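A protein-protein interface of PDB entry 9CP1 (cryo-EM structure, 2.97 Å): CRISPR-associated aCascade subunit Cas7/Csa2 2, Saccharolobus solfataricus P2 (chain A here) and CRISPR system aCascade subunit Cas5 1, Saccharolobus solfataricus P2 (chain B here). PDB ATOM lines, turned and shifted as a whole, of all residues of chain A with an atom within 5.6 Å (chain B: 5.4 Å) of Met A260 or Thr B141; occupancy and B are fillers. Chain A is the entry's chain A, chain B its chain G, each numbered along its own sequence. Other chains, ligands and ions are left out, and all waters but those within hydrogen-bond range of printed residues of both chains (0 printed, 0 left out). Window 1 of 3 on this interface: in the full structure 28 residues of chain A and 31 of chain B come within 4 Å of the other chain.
Among the printed residues, pairs that only touch across the chains: Met A260 with Thr B141, Met A260 with Ala B150, Arg A276 with Ser B151, Pro A261 with His B11 and Met A260 with Leu B149.
A ring nitrogen (NE2) of His B11 is in hydrogen-bond range of the side-chain hydroxyl (OG) of Ser B151 (3.3 Å). The backbone NH (N) of Ala B150 lies within hydrogen-bond range of the backbone carbonyl oxygen (O) of Thr B141 (3.0 Å). OE2 of Glu A262 is in salt-bridge range of NE of Arg A276 (2.5 Å). The backbone carbonyl oxygen (O) of Met A260 sits at hydrogen-bond distance from the guanidinium group (NH2) of Arg A276, at 3.0 Å.
O of Pro A261 lies within hydrogen-bond range of OG of Ser B151.
Met A260 touches just these residues of chain B: Thr B141 (3.1 Å), Leu B149 (3.9 Å) and Ala B150 (3.2 Å). Of chain A, only Met A260 (3.1 Å) comes within 4 Å of Thr B141. Printed residues of chain A within 4 Å of His B11: Pro A261 (3.8 Å). Printed residues of chain A within 4 Å of Leu B149: Met A260 (3.9 Å). Printed residues of chain B within 4 Å of Arg A276: Ser B151. Printed residues of chain A within 4 Å of Ala B150: Met A260. Of the printed residues of chain A, Ser B151 touches Pro A261 and Arg A276. Ile B143 touches none of the printed residues of chain A. The nearest residue of chain B that does not touch Met A260 is Ser B151 (4.2 Å).
Of the 10 printed residues of chain A, 3 touch a printed residue of chain B. Printed residues of chain A that touch a printed residue of chain B: Met A260, Pro A261 and Arg A276. Along chain A the printed residues that touch a printed residue of chain B span positions 260 to 276. Hydrophobic or aromatic side chains of chain B that line the printed part of chain A: His B11 and Leu B149. Along chain B the printed residues that touch a printed residue of chain A span positions 11 to 151. Among the printed residues, no Asp or Glu carboxylate lies within 4 Å of a Lys or Arg side-chain nitrogen of the other chain.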
ATOM      1  N   MET A   1     -12.016  12.534  -9.217  1.00  0.00           N
ATOM      2  CA  MET A   1     -11.516  12.167  -7.899  1.00  0.00           C
ATOM      3  C   MET A   1     -10.858  13.347  -7.202  1.00  0.00           C
ATOM      4  O   MET A   1     -10.622  14.389  -7.807  1.00  0.00           O
ATOM      5  CB  MET A   1     -10.519  11.015  -8.002  1.00  0.00           C
ATOM      6  CG  MET A   1     -11.130   9.649  -7.783  1.00  0.00           C
ATOM      7  SD  MET A   1      -9.992   8.316  -8.196  1.00  0.00           S
ATOM      8  CE  MET A   1      -8.470   8.964  -7.518  1.00  0.00           C
ATOM      9  N   SER A   3      -7.509  14.067  -4.532  1.00  0.00           N
ATOM     10  CA  SER A   3      -6.313  13.515  -3.920  1.00  0.00           C
ATOM     11  C   SER A   3      -5.626  14.601  -3.112  1.00  0.00           C
ATOM     12  O   SER A   3      -5.677  15.778  -3.470  1.00  0.00           O
ATOM     13  CB  SER A   3      -5.354  12.958  -4.973  1.00  0.00           C
ATOM     14  OG  SER A   3      -5.940  11.869  -5.661  1.00  0.00           O
ATOM     15  N   GLU A 189      -7.062   9.829  -0.436  1.00  0.00           N
ATOM     16  CA  GLU A 189      -7.781   9.781  -1.702  1.00  0.00           C
ATOM     17  C   GLU A 189      -9.275   9.649  -1.439  1.00  0.00           C
ATOM     18  O   GLU A 189      -9.695   8.969  -0.502  1.00  0.00           O
ATOM     19  CB  GLU A 189      -7.301   8.612  -2.572  1.00  0.00           C
ATOM     20  CG  GLU A 189      -8.135   8.376  -3.818  1.00  0.00           C
ATOM     21  CD  GLU A 189      -7.668   7.182  -4.619  1.00  0.00           C
ATOM     22  OE1 GLU A 189      -6.455   6.890  -4.603  1.00  0.00           O
ATOM     23  OE2 GLU A 189      -8.515   6.536  -5.270  1.00  0.00           O
ATOM     24  N   PRO A 258      -7.624   8.423 -12.510  1.00  0.00           N
ATOM     25  CA  PRO A 258      -6.768   8.077 -11.369  1.00  0.00           C
ATOM     26  C   PRO A 258      -5.465   8.866 -11.375  1.00  0.00           C
ATOM     27  O   PRO A 258      -4.826   9.038 -12.415  1.00  0.00           O
ATOM     28  CB  PRO A 258      -6.517   6.577 -11.557  1.00  0.00           C
ATOM     29  CG  PRO A 258      -7.663   6.103 -12.367  1.00  0.00           C
ATOM     30  CD  PRO A 258      -8.015   7.231 -13.282  1.00  0.00           C
ATOM     31  N   PHE A 259      -5.071   9.327 -10.191  1.00  0.00           N
ATOM     32  CA  PHE A 259      -3.856  10.107  -9.991  1.00  0.00           C
ATOM     33  C   PHE A 259      -3.653  10.316  -8.500  1.00  0.00           C
ATOM     34  O   PHE A 259      -4.620  10.383  -7.738  1.00  0.00           O
ATOM     35  CB  PHE A 259      -3.931  11.461 -10.705  1.00  0.00           C
ATOM     36  CG  PHE A 259      -2.733  12.332 -10.475  1.00  0.00           C
ATOM     37  CD1 PHE A 259      -1.563  12.124 -11.179  1.00  0.00           C
ATOM     38  CD2 PHE A 259      -2.780  13.359  -9.553  1.00  0.00           C
ATOM     39  CE1 PHE A 259      -0.464  12.925 -10.964  1.00  0.00           C
ATOM     40  CE2 PHE A 259      -1.685  14.162  -9.335  1.00  0.00           C
ATOM     41  CZ  PHE A 259      -0.527  13.944 -10.042  1.00  0.00           C
ATOM     42  N   MET A 260      -2.391  10.419  -8.095  1.00  0.00           N
ATOM     43  CA  MET A 260      -2.041  10.754  -6.723  1.00  0.00           C
ATOM     44  C   MET A 260      -0.785  11.610  -6.709  1.00  0.00           C
ATOM     45  O   MET A 260       0.047  11.513  -7.619  1.00  0.00           O
ATOM     46  CB  MET A 260      -1.817   9.501  -5.865  1.00  0.00           C
ATOM     47  CG  MET A 260      -3.090   8.914  -5.302  1.00  0.00           C
ATOM     48  SD  MET A 260      -2.729   7.502  -4.262  1.00  0.00           S
ATOM     49  CE  MET A 260      -1.816   6.516  -5.437  1.00  0.00           C
ATOM     50  N   PRO A 261      -0.622  12.454  -5.698  1.00  0.00           N
ATOM     51  CA  PRO A 261       0.571  13.293  -5.603  1.00  0.00           C
ATOM     52  C   PRO A 261       1.720  12.577  -4.902  1.00  0.00           C
ATOM     53  O   PRO A 261       1.573  11.482  -4.358  1.00  0.00           O
ATOM     54  CB  PRO A 261       0.092  14.496  -4.779  1.00  0.00           C
ATOM     55  CG  PRO A 261      -1.087  14.019  -4.024  1.00  0.00           C
ATOM     56  CD  PRO A 261      -1.622  12.778  -4.668  1.00  0.00           C
ATOM     57  N   GLU A 262       2.879  13.225  -4.936  1.00  0.00           N
ATOM     58  CA  GLU A 262       4.063  12.678  -4.299  1.00  0.00           C
ATOM     59  C   GLU A 262       3.926  12.735  -2.779  1.00  0.00           C
ATOM     60  O   GLU A 262       3.243  13.611  -2.242  1.00  0.00           O
ATOM     61  CB  GLU A 262       5.305  13.455  -4.729  1.00  0.00           C
ATOM     62  CG  GLU A 262       5.570  13.432  -6.221  1.00  0.00           C
ATOM     63  CD  GLU A 262       6.300  12.180  -6.661  1.00  0.00           C
ATOM     64  OE1 GLU A 262       6.655  11.360  -5.790  1.00  0.00           O
ATOM     65  OE2 GLU A 262       6.522  12.016  -7.878  1.00  0.00           O
ATOM     66  N   THR A 273       4.759  16.973  -8.292  1.00  0.00           N
ATOM     67  CA  THR A 273       3.398  16.512  -8.524  1.00  0.00           C
ATOM     68  C   THR A 273       2.705  17.335  -9.600  1.00  0.00           C
ATOM     69  O   THR A 273       1.881  16.797 -10.339  1.00  0.00           O
ATOM     70  CB  THR A 273       2.586  16.515  -7.225  1.00  0.00           C
ATOM     71  OG1 THR A 273       1.339  15.848  -7.450  1.00  0.00           O
ATOM     72  CG2 THR A 273       2.299  17.919  -6.750  1.00  0.00           C
ATOM     73  N   ARG A 276       4.064  15.857 -12.861  1.00  0.00           N
ATOM     74  CA  ARG A 276       3.479  14.544 -13.096  1.00  0.00           C
ATOM     75  C   ARG A 276       1.997  14.637 -13.431  1.00  0.00           C
ATOM     76  O   ARG A 276       1.497  13.836 -14.223  1.00  0.00           O
ATOM     77  CB  ARG A 276       3.700  13.647 -11.883  1.00  0.00           C
ATOM     78  CG  ARG A 276       5.135  13.180 -11.737  1.00  0.00           C
ATOM     79  CD  ARG A 276       5.229  11.949 -10.859  1.00  0.00           C
ATOM     80  NE  ARG A 276       4.615  12.168  -9.557  1.00  0.00           N
ATOM     81  CZ  ARG A 276       3.491  11.592  -9.154  1.00  0.00           C
ATOM     82  NH1 ARG A 276       2.838  10.737  -9.924  1.00  0.00           N
ATOM     83  NH2 ARG A 276       3.008  11.885  -7.950  1.00  0.00           N
ATOM     84  N   HIS B  11       4.396   5.346  -0.018  1.00  0.00           N
ATOM     85  CA  HIS B  11       4.139   6.347   1.011  1.00  0.00           C
ATOM     86  C   HIS B  11       4.644   5.893   2.377  1.00  0.00           C
ATOM     87  O   HIS B  11       5.395   6.619   3.035  1.00  0.00           O
ATOM     88  CB  HIS B  11       2.644   6.676   1.053  1.00  0.00           C
ATOM     89  CG  HIS B  11       2.173   7.461  -0.130  1.00  0.00           C
ATOM     90  ND1 HIS B  11       1.944   8.819  -0.078  1.00  0.00           N
ATOM     91  CD2 HIS B  11       1.904   7.083  -1.402  1.00  0.00           C
ATOM     92  CE1 HIS B  11       1.547   9.242  -1.264  1.00  0.00           C
ATOM     93  NE2 HIS B  11       1.514   8.209  -2.085  1.00  0.00           N
ATOM     94  N   TYR B  42      -6.897  -2.976 -11.832  1.00  0.00           N
ATOM     95  CA  TYR B  42      -7.693  -1.905 -11.237  1.00  0.00           C
ATOM     96  C   TYR B  42      -7.952  -0.769 -12.218  1.00  0.00           C
ATOM     97  O   TYR B  42      -8.986  -0.100 -12.128  1.00  0.00           O
ATOM     98  CB  TYR B  42      -7.001  -1.367  -9.983  1.00  0.00           C
ATOM     99  CG  TYR B  42      -7.558  -0.051  -9.479  1.00  0.00           C
ATOM    100  CD1 TYR B  42      -8.643  -0.020  -8.617  1.00  0.00           C
ATOM    101  CD2 TYR B  42      -6.988   1.158  -9.851  1.00  0.00           C
ATOM    102  CE1 TYR B  42      -9.152   1.176  -8.152  1.00  0.00           C
ATOM    103  CE2 TYR B  42      -7.492   2.356  -9.392  1.00  0.00           C
ATOM    104  CZ  TYR B  42      -8.572   2.360  -8.542  1.00  0.00           C
ATOM    105  OH  TYR B  42      -9.075   3.554  -8.081  1.00  0.00           O
ATOM    106  N   SER B 139      -2.253   3.775 -14.314  1.00  0.00           N
ATOM    107  CA  SER B 139      -3.457   3.782 -13.482  1.00  0.00           C
ATOM    108  C   SER B 139      -3.332   2.886 -12.255  1.00  0.00           C
ATOM    109  O   SER B 139      -4.269   2.157 -11.921  1.00  0.00           O
ATOM    110  CB  SER B 139      -4.666   3.377 -14.316  1.00  0.00           C
ATOM    111  OG  SER B 139      -4.788   4.196 -15.466  1.00  0.00           O
ATOM    112  N   ILE B 140      -2.196   2.909 -11.564  1.00  0.00           N
ATOM    113  CA  ILE B 140      -1.985   2.110 -10.361  1.00  0.00           C
ATOM    114  C   ILE B 140      -2.047   3.025  -9.146  1.00  0.00           C
ATOM    115  O   ILE B 140      -1.414   4.088  -9.128  1.00  0.00           O
ATOM    116  CB  ILE B 140      -0.645   1.358 -10.420  1.00  0.00           C
ATOM    117  CG1 ILE B 140      -0.754   0.157 -11.358  1.00  0.00           C
ATOM    118  CG2 ILE B 140      -0.215   0.910  -9.036  1.00  0.00           C
ATOM    119  CD1 ILE B 140       0.579  -0.428 -11.754  1.00  0.00           C
ATOM    120  N   THR B 141      -2.808   2.617  -8.129  1.00  0.00           N
ATOM    121  CA  THR B 141      -3.006   3.438  -6.940  1.00  0.00           C
ATOM    122  C   THR B 141      -2.540   2.793  -5.644  1.00  0.00           C
ATOM    123  O   THR B 141      -2.065   3.507  -4.760  1.00  0.00           O
ATOM    124  CB  THR B 141      -4.485   3.815  -6.792  1.00  0.00           C
ATOM    125  OG1 THR B 141      -5.300   2.660  -7.026  1.00  0.00           O
ATOM    126  CG2 THR B 141      -4.857   4.910  -7.780  1.00  0.00           C
ATOM    127  N   ARG B 142      -2.657   1.479  -5.493  1.00  0.00           N
ATOM    128  CA  ARG B 142      -2.216   0.862  -4.250  1.00  0.00           C
ATOM    129  C   ARG B 142      -1.795  -0.572  -4.519  1.00  0.00           C
ATOM    130  O   ARG B 142      -2.130  -1.156  -5.552  1.00  0.00           O
ATOM    131  CB  ARG B 142      -3.306   0.896  -3.177  1.00  0.00           C
ATOM    132  CG  ARG B 142      -4.505   0.038  -3.504  1.00  0.00           C
ATOM    133  CD  ARG B 142      -5.586   0.160  -2.452  1.00  0.00           C
ATOM    134  NE  ARG B 142      -6.781  -0.590  -2.816  1.00  0.00           N
ATOM    135  CZ  ARG B 142      -7.027  -1.834  -2.432  1.00  0.00           C
ATOM    136  NH1 ARG B 142      -6.169  -2.508  -1.684  1.00  0.00           N
ATOM    137  NH2 ARG B 142      -8.159  -2.419  -2.811  1.00  0.00           N
ATOM    138  N   ILE B 143      -1.053  -1.129  -3.566  1.00  0.00           N
ATOM    139  CA  ILE B 143      -0.576  -2.505  -3.622  1.00  0.00           C
ATOM    140  C   ILE B 143      -0.889  -3.149  -2.279  1.00  0.00           C
ATOM    141  O   ILE B 143      -0.250  -2.829  -1.271  1.00  0.00           O
ATOM    142  CB  ILE B 143       0.924  -2.585  -3.932  1.00  0.00           C
ATOM    143  CG1 ILE B 143       1.194  -2.128  -5.364  1.00  0.00           C
ATOM    144  CG2 ILE B 143       1.438  -3.995  -3.715  1.00  0.00           C
ATOM    145  CD1 ILE B 143       2.627  -1.740  -5.618  1.00  0.00           C
ATOM    146  N   CYS B 148      -1.907   1.277   1.698  1.00  0.00           N
ATOM    147  CA  CYS B 148      -0.644   1.183   0.965  1.00  0.00           C
ATOM    148  C   CYS B 148      -0.729   1.913  -0.376  1.00  0.00           C
ATOM    149  O   CYS B 148      -0.609   1.327  -1.449  1.00  0.00           O
ATOM    150  CB  CYS B 148      -0.263  -0.279   0.776  1.00  0.00           C
ATOM    151  SG  CYS B 148      -0.514  -1.287   2.246  1.00  0.00           S
ATOM    152  N   LEU B 149      -0.930   3.224  -0.296  1.00  0.00           N
ATOM    153  CA  LEU B 149      -0.951   4.048  -1.495  1.00  0.00           C
ATOM    154  C   LEU B 149       0.441   4.129  -2.108  1.00  0.00           C
ATOM    155  O   LEU B 149       1.455   3.967  -1.424  1.00  0.00           O
ATOM    156  CB  LEU B 149      -1.467   5.447  -1.169  1.00  0.00           C
ATOM    157  CG  LEU B 149      -2.702   5.500  -0.271  1.00  0.00           C
ATOM    158  CD1 LEU B 149      -2.930   6.908   0.238  1.00  0.00           C
ATOM    159  CD2 LEU B 149      -3.923   5.004  -1.022  1.00  0.00           C
ATOM    160  N   ALA B 150       0.488   4.381  -3.417  1.00  0.00           N
ATOM    161  CA  ALA B 150       1.762   4.394  -4.135  1.00  0.00           C
ATOM    162  C   ALA B 150       1.613   5.244  -5.389  1.00  0.00           C
ATOM    163  O   ALA B 150       0.797   4.923  -6.258  1.00  0.00           O
ATOM    164  CB  ALA B 150       2.196   2.976  -4.483  1.00  0.00           C
ATOM    165  N   SER B 151       2.405   6.308  -5.485  1.00  0.00           N
ATOM    166  CA  SER B 151       2.394   7.176  -6.651  1.00  0.00           C
ATOM    167  C   SER B 151       3.138   6.526  -7.816  1.00  0.00           C
ATOM    168  O   SER B 151       3.816   5.507  -7.667  1.00  0.00           O
ATOM    169  CB  SER B 151       3.016   8.529  -6.315  1.00  0.00           C
ATOM    170  OG  SER B 151       2.421   9.086  -5.158  1.00  0.00           O
